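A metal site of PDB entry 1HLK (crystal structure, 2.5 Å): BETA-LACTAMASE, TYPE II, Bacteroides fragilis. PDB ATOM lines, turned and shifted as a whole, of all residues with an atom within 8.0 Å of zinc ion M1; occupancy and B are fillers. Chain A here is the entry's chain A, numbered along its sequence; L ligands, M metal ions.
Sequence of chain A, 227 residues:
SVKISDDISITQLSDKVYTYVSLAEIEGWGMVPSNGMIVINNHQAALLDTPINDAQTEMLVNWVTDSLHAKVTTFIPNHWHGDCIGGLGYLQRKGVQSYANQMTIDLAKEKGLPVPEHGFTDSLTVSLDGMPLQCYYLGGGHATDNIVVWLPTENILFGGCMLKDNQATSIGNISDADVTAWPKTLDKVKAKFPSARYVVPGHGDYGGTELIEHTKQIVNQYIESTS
The side-chain amide oxygen (OD1) of Asn 146 sits at hydrogen-bond distance from the backbone NH (N) of His 142, at 3.1 Å. ND1 of His 79 lies close to SG of Cys 84, at 3.4 Å. A ring nitrogen (ND1) of His 79 sits at hydrogen-bond distance from the side-chain amide oxygen (OD1) of Asn 78, at 2.7 Å. NE2 of His 81 is in hydrogen-bond range of OD2 of Asp 176 (2.7 Å).
Of the 18 residues printed, 3 come within 4 Å of zinc ion M1. The nearest printed residue that does not touch zinc ion M1 is Asp 83 (4.1 Å).
The backbone NH (N) of Asn 173 sits at hydrogen-bond distance from an oxygen (O7) of the ligand, 3.1 Å away. The side-chain amide nitrogen (ND2) of Asn 173 lies within hydrogen-bond range of an oxygen (O3) of the ligand (3.4 Å).
NE2 of His 142 binds zinc ion M1. Zinc ion M1 is bound by a ring nitrogen (NE2) of His 79, 2.2 Å away. ND1 of His 81 binds zinc ion M1 (2.3 Å). Zinc ion M1 has three donor atoms within binding distance.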
ATOM      1  N   ASP A  49     -23.361  23.241  20.169  1.00  0.00           N
ATOM      2  CA  ASP A  49     -23.431  23.495  21.598  1.00  0.00           C
ATOM      3  C   ASP A  49     -24.562  24.477  21.851  1.00  0.00           C
ATOM      4  O   ASP A  49     -24.859  25.329  21.011  1.00  0.00           O
ATOM      5  CB  ASP A  49     -22.122  24.092  22.118  1.00  0.00           C
ATOM      6  CG  ASP A  49     -21.040  23.060  22.288  1.00  0.00           C
ATOM      7  OD1 ASP A  49     -21.045  22.083  21.528  1.00  0.00           O
ATOM      8  OD2 ASP A  49     -20.176  23.242  23.176  1.00  0.00           O
ATOM      9  N   ASN A  78     -20.753  19.164  21.670  1.00  0.00           N
ATOM     10  CA  ASN A  78     -19.342  18.794  21.754  1.00  0.00           C
ATOM     11  C   ASN A  78     -19.152  17.539  22.609  1.00  0.00           C
ATOM     12  O   ASN A  78     -18.313  16.676  22.282  1.00  0.00           O
ATOM     13  CB  ASN A  78     -18.511  19.949  22.310  1.00  0.00           C
ATOM     14  CG  ASN A  78     -17.016  19.663  22.280  1.00  0.00           C
ATOM     15  OD1 ASN A  78     -16.468  19.031  23.176  1.00  0.00           O
ATOM     16  ND2 ASN A  78     -16.369  20.108  21.220  1.00  0.00           N
ATOM     17  N   HIS A  79     -19.908  17.465  23.699  1.00  0.00           N
ATOM     18  CA  HIS A  79     -19.914  16.317  24.604  1.00  0.00           C
ATOM     19  C   HIS A  79     -21.100  16.441  25.584  1.00  0.00           C
ATOM     20  O   HIS A  79     -21.857  17.411  25.521  1.00  0.00           O
ATOM     21  CB  HIS A  79     -18.569  16.140  25.342  1.00  0.00           C
ATOM     22  CG  HIS A  79     -18.117  17.324  26.121  1.00  0.00           C
ATOM     23  ND1 HIS A  79     -17.772  18.524  25.528  1.00  0.00           N
ATOM     24  CD2 HIS A  79     -17.987  17.526  27.453  1.00  0.00           C
ATOM     25  CE1 HIS A  79     -17.449  19.406  26.467  1.00  0.00           C
ATOM     26  NE2 HIS A  79     -17.573  18.819  27.641  1.00  0.00           N
ATOM     27  N   TRP A  80     -21.265  15.461  26.463  1.00  0.00           N
ATOM     28  CA  TRP A  80     -22.391  15.433  27.387  1.00  0.00           C
ATOM     29  C   TRP A  80     -22.576  16.467  28.492  1.00  0.00           C
ATOM     30  O   TRP A  80     -23.617  16.434  29.158  1.00  0.00           O
ATOM     31  CB  TRP A  80     -22.496  14.061  28.059  1.00  0.00           C
ATOM     32  CG  TRP A  80     -21.358  13.748  28.983  1.00  0.00           C
ATOM     33  CD1 TRP A  80     -20.107  13.349  28.630  1.00  0.00           C
ATOM     34  CD2 TRP A  80     -21.371  13.810  30.410  1.00  0.00           C
ATOM     35  NE1 TRP A  80     -19.334  13.160  29.752  1.00  0.00           N
ATOM     36  CE2 TRP A  80     -20.089  13.431  30.864  1.00  0.00           C
ATOM     37  CE3 TRP A  80     -22.349  14.153  31.361  1.00  0.00           C
ATOM     38  CZ2 TRP A  80     -19.752  13.383  32.226  1.00  0.00           C
ATOM     39  CZ3 TRP A  80     -22.016  14.113  32.719  1.00  0.00           C
ATOM     40  CH2 TRP A  80     -20.725  13.723  33.135  1.00  0.00           C
ATOM     41  N   HIS A  81     -21.629  17.379  28.689  1.00  0.00           N
ATOM     42  CA  HIS A  81     -21.765  18.374  29.753  1.00  0.00           C
ATOM     43  C   HIS A  81     -22.818  19.439  29.537  1.00  0.00           C
ATOM     44  O   HIS A  81     -23.301  19.650  28.423  1.00  0.00           O
ATOM     45  CB  HIS A  81     -20.423  19.028  30.081  1.00  0.00           C
ATOM     46  CG  HIS A  81     -19.513  18.154  30.880  1.00  0.00           C
ATOM     47  ND1 HIS A  81     -18.161  18.420  31.020  1.00  0.00           N
ATOM     48  CD2 HIS A  81     -19.749  17.034  31.592  1.00  0.00           C
ATOM     49  CE1 HIS A  81     -17.617  17.494  31.792  1.00  0.00           C
ATOM     50  NE2 HIS A  81     -18.555  16.638  32.148  1.00  0.00           N
ATOM     51  N   GLY A  82     -23.176  20.100  30.642  1.00  0.00           N
ATOM     52  CA  GLY A  82     -24.189  21.141  30.626  1.00  0.00           C
ATOM     53  C   GLY A  82     -23.977  22.229  29.596  1.00  0.00           C
ATOM     54  O   GLY A  82     -24.920  22.682  28.952  1.00  0.00           O
ATOM     55  N   ASP A  83     -22.727  22.649  29.438  1.00  0.00           N
ATOM     56  CA  ASP A  83     -22.412  23.696  28.488  1.00  0.00           C
ATOM     57  C   ASP A  83     -22.341  23.230  27.028  1.00  0.00           C
ATOM     58  O   ASP A  83     -21.721  23.878  26.178  1.00  0.00           O
ATOM     59  CB  ASP A  83     -21.119  24.404  28.916  1.00  0.00           C
ATOM     60  CG  ASP A  83     -19.988  23.452  29.255  1.00  0.00           C
ATOM     61  OD1 ASP A  83     -20.202  22.556  30.107  1.00  0.00           O
ATOM     62  OD2 ASP A  83     -18.883  23.602  28.685  1.00  0.00           O
ATOM     63  N   CYS A  84     -22.997  22.111  26.739  1.00  0.00           N
ATOM     64  CA  CYS A  84     -23.040  21.575  25.382  1.00  0.00           C
ATOM     65  C   CYS A  84     -24.483  21.207  24.994  1.00  0.00           C
ATOM     66  O   CYS A  84     -24.970  21.615  23.936  1.00  0.00           O
ATOM     67  CB  CYS A  84     -22.119  20.367  25.257  1.00  0.00           C
ATOM     68  SG  CYS A  84     -20.403  20.684  25.703  1.00  0.00           S
ATOM     69  N   HIS A 142     -10.698  16.349  27.223  1.00  0.00           N
ATOM     70  CA  HIS A 142     -11.402  17.022  28.307  1.00  0.00           C
ATOM     71  C   HIS A 142     -12.453  16.067  28.840  1.00  0.00           C
ATOM     72  O   HIS A 142     -12.717  16.003  30.032  1.00  0.00           O
ATOM     73  CB  HIS A 142     -12.100  18.277  27.804  1.00  0.00           C
ATOM     74  CG  HIS A 142     -13.172  18.761  28.721  1.00  0.00           C
ATOM     75  ND1 HIS A 142     -12.915  19.281  29.962  1.00  0.00           N
ATOM     76  CD2 HIS A 142     -14.525  18.707  28.611  1.00  0.00           C
ATOM     77  CE1 HIS A 142     -14.048  19.523  30.585  1.00  0.00           C
ATOM     78  NE2 HIS A 142     -15.048  19.191  29.786  1.00  0.00           N
ATOM     79  N   ALA A 143     -13.070  15.341  27.911  1.00  0.00           N
ATOM     80  CA  ALA A 143     -14.103  14.376  28.204  1.00  0.00           C
ATOM     81  C   ALA A 143     -13.792  13.155  27.348  1.00  0.00           C
ATOM     82  O   ALA A 143     -13.027  13.239  26.408  1.00  0.00           O
ATOM     83  CB  ALA A 143     -15.470  14.965  27.858  1.00  0.00           C
ATOM     84  N   ASP A 145     -15.930  11.541  25.446  1.00  0.00           N
ATOM     85  CA  ASP A 145     -16.714  11.602  24.221  1.00  0.00           C
ATOM     86  C   ASP A 145     -16.499  12.810  23.316  1.00  0.00           C
ATOM     87  O   ASP A 145     -17.069  12.855  22.222  1.00  0.00           O
ATOM     88  CB  ASP A 145     -18.212  11.501  24.554  1.00  0.00           C
ATOM     89  CG  ASP A 145     -18.701  12.603  25.512  1.00  0.00           C
ATOM     90  OD1 ASP A 145     -19.795  13.158  25.263  1.00  0.00           O
ATOM     91  OD2 ASP A 145     -18.029  12.902  26.522  1.00  0.00           O
ATOM     92  N   ASN A 146     -15.712  13.776  23.758  1.00  0.00           N
ATOM     93  CA  ASN A 146     -15.481  15.005  22.990  1.00  0.00           C
ATOM     94  C   ASN A 146     -15.051  14.875  21.510  1.00  0.00           C
ATOM     95  O   ASN A 146     -14.181  14.081  21.158  1.00  0.00           O
ATOM     96  CB  ASN A 146     -14.484  15.908  23.738  1.00  0.00           C
ATOM     97  CG  ASN A 146     -13.066  15.313  23.840  1.00  0.00           C
ATOM     98  OD1 ASN A 146     -12.207  15.889  24.507  1.00  0.00           O
ATOM     99  ND2 ASN A 146     -12.838  14.172  23.187  1.00  0.00           N
ATOM    100  N   GLY A 160     -14.082  22.942  21.005  1.00  0.00           N
ATOM    101  CA  GLY A 160     -14.725  22.629  22.272  1.00  0.00           C
ATOM    102  C   GLY A 160     -13.771  22.814  23.438  1.00  0.00           C
ATOM    103  O   GLY A 160     -12.792  23.560  23.362  1.00  0.00           O
ATOM    104  N   CYS A 161     -14.036  22.119  24.527  1.00  0.00           N
ATOM    105  CA  CYS A 161     -13.232  22.241  25.720  1.00  0.00           C
ATOM    106  C   CYS A 161     -11.947  21.447  25.713  1.00  0.00           C
ATOM    107  O   CYS A 161     -11.175  21.485  26.678  1.00  0.00           O
ATOM    108  CB  CYS A 161     -14.093  21.884  26.949  1.00  0.00           C
ATOM    109  SG  CYS A 161     -15.562  22.952  27.085  1.00  0.00           S
ATOM    110  N   MET A 162     -11.684  20.709  24.642  1.00  0.00           N
ATOM    111  CA  MET A 162     -10.403  20.000  24.639  1.00  0.00           C
ATOM    112  C   MET A 162      -9.342  21.054  24.368  1.00  0.00           C
ATOM    113  O   MET A 162      -8.173  20.856  24.653  1.00  0.00           O
ATOM    114  CB  MET A 162     -10.339  18.895  23.560  1.00  0.00           C
ATOM    115  CG  MET A 162      -9.979  19.341  22.153  1.00  0.00           C
ATOM    116  SD  MET A 162      -9.600  17.922  21.128  1.00  0.00           S
ATOM    117  CE  MET A 162     -11.144  16.967  21.222  1.00  0.00           C
ATOM    118  N   ASN A 173     -11.503  21.927  34.742  1.00  0.00           N
ATOM    119  CA  ASN A 173     -12.333  20.822  35.235  1.00  0.00           C
ATOM    120  C   ASN A 173     -11.981  19.476  34.599  1.00  0.00           C
ATOM    121  O   ASN A 173     -12.501  19.122  33.545  1.00  0.00           O
ATOM    122  CB  ASN A 173     -13.808  21.137  34.970  1.00  0.00           C
ATOM    123  CG  ASN A 173     -14.731  20.017  35.413  1.00  0.00           C
ATOM    124  OD1 ASN A 173     -14.742  19.631  36.583  1.00  0.00           O
ATOM    125  ND2 ASN A 173     -15.514  19.490  34.480  1.00  0.00           N
ATOM    126  N   ASP A 176     -14.074  14.464  34.272  1.00  0.00           N
ATOM    127  CA  ASP A 176     -14.481  13.431  33.328  1.00  0.00           C
ATOM    128  C   ASP A 176     -13.408  13.327  32.261  1.00  0.00           C
ATOM    129  O   ASP A 176     -13.578  12.661  31.247  1.00  0.00           O
ATOM    130  CB  ASP A 176     -15.796  13.822  32.669  1.00  0.00           C
ATOM    131  CG  ASP A 176     -16.916  13.953  33.663  1.00  0.00           C
ATOM    132  OD1 ASP A 176     -17.366  12.914  34.171  1.00  0.00           O
ATOM    133  OD2 ASP A 176     -17.336  15.091  33.950  1.00  0.00           O
ATOM    134  N   HIS A 203     -14.109  27.665  26.001  1.00  0.00           N
ATOM    135  CA  HIS A 203     -14.139  28.762  26.962  1.00  0.00           C
ATOM    136  C   HIS A 203     -12.978  29.692  26.646  1.00  0.00           C
ATOM    137  O   HIS A 203     -11.853  29.233  26.517  1.00  0.00           O
ATOM    138  CB  HIS A 203     -13.972  28.254  28.405  1.00  0.00           C
ATOM    139  CG  HIS A 203     -15.099  27.372  28.865  1.00  0.00           C
ATOM    140  ND1 HIS A 203     -16.353  27.858  29.169  1.00  0.00           N
ATOM    141  CD2 HIS A 203     -15.166  26.035  29.041  1.00  0.00           C
ATOM    142  CE1 HIS A 203     -17.142  26.854  29.500  1.00  0.00           C
ATOM    143  NE2 HIS A 203     -16.444  25.740  29.432  1.00  0.00           N
HETATM  144  C1  LIG L   1     -16.481  24.087  33.891  1.00  0.00           C
HETATM  145  C2  LIG L   1     -15.995  25.227  34.531  1.00  0.00           C
HETATM  146  C3  LIG L   1     -14.892  25.881  34.008  1.00  0.00           C
HETATM  147  C4  LIG L   1     -14.223  25.365  32.877  1.00  0.00           C
HETATM  148  C5  LIG L   1     -14.511  24.035  32.472  1.00  0.00           C
HETATM  149  C6  LIG L   1     -15.702  23.435  32.925  1.00  0.00           C
HETATM  150  O1  LIG L   1     -14.456  27.049  34.605  1.00  0.00           O
HETATM  151  C7  LIG L   1     -13.356  27.742  34.145  1.00  0.00           C
HETATM  152  C8  LIG L   1     -12.742  27.438  32.978  1.00  0.00           C
HETATM  153  C9  LIG L   1     -13.271  26.266  32.187  1.00  0.00           C
HETATM  154  C10 LIG L   1     -12.897  28.848  35.046  1.00  0.00           C
HETATM  155  C11 LIG L   1     -11.420  29.189  34.806  1.00  0.00           C
HETATM  156  O2  LIG L   1     -11.139  29.281  33.404  1.00  0.00           O
HETATM  157  C12 LIG L   1     -11.553  28.256  32.488  1.00  0.00           C
HETATM  158  O3  LIG L   1     -16.178  22.205  32.488  1.00  0.00           O
HETATM  159  O4  LIG L   1     -17.726  23.553  34.150  1.00  0.00           O
HETATM  160  C13 LIG L   1     -13.614  23.257  31.595  1.00  0.00           C
HETATM  161  O5  LIG L   1     -13.983  23.216  30.297  1.00  0.00           O
HETATM  162  O6  LIG L   1     -10.457  27.463  32.039  1.00  0.00           O
HETATM  163  C14 LIG L   1      -9.550  26.874  32.952  1.00  0.00           C
HETATM  164  C15 LIG L   1     -10.980  30.499  35.468  1.00  0.00           C
HETATM  165  O7  LIG L   1     -12.620  22.718  32.009  1.00  0.00           O
HETATM  166  O8  LIG L   1     -12.913  26.131  31.036  1.00  0.00           O
HETATM  167 ZN    ZN M   1     -17.149  19.863  29.553  1.00  0.00          ZN
HETATM  168 ZN    ZN M   2     -16.221  23.033  29.084  1.00  0.00          ZN
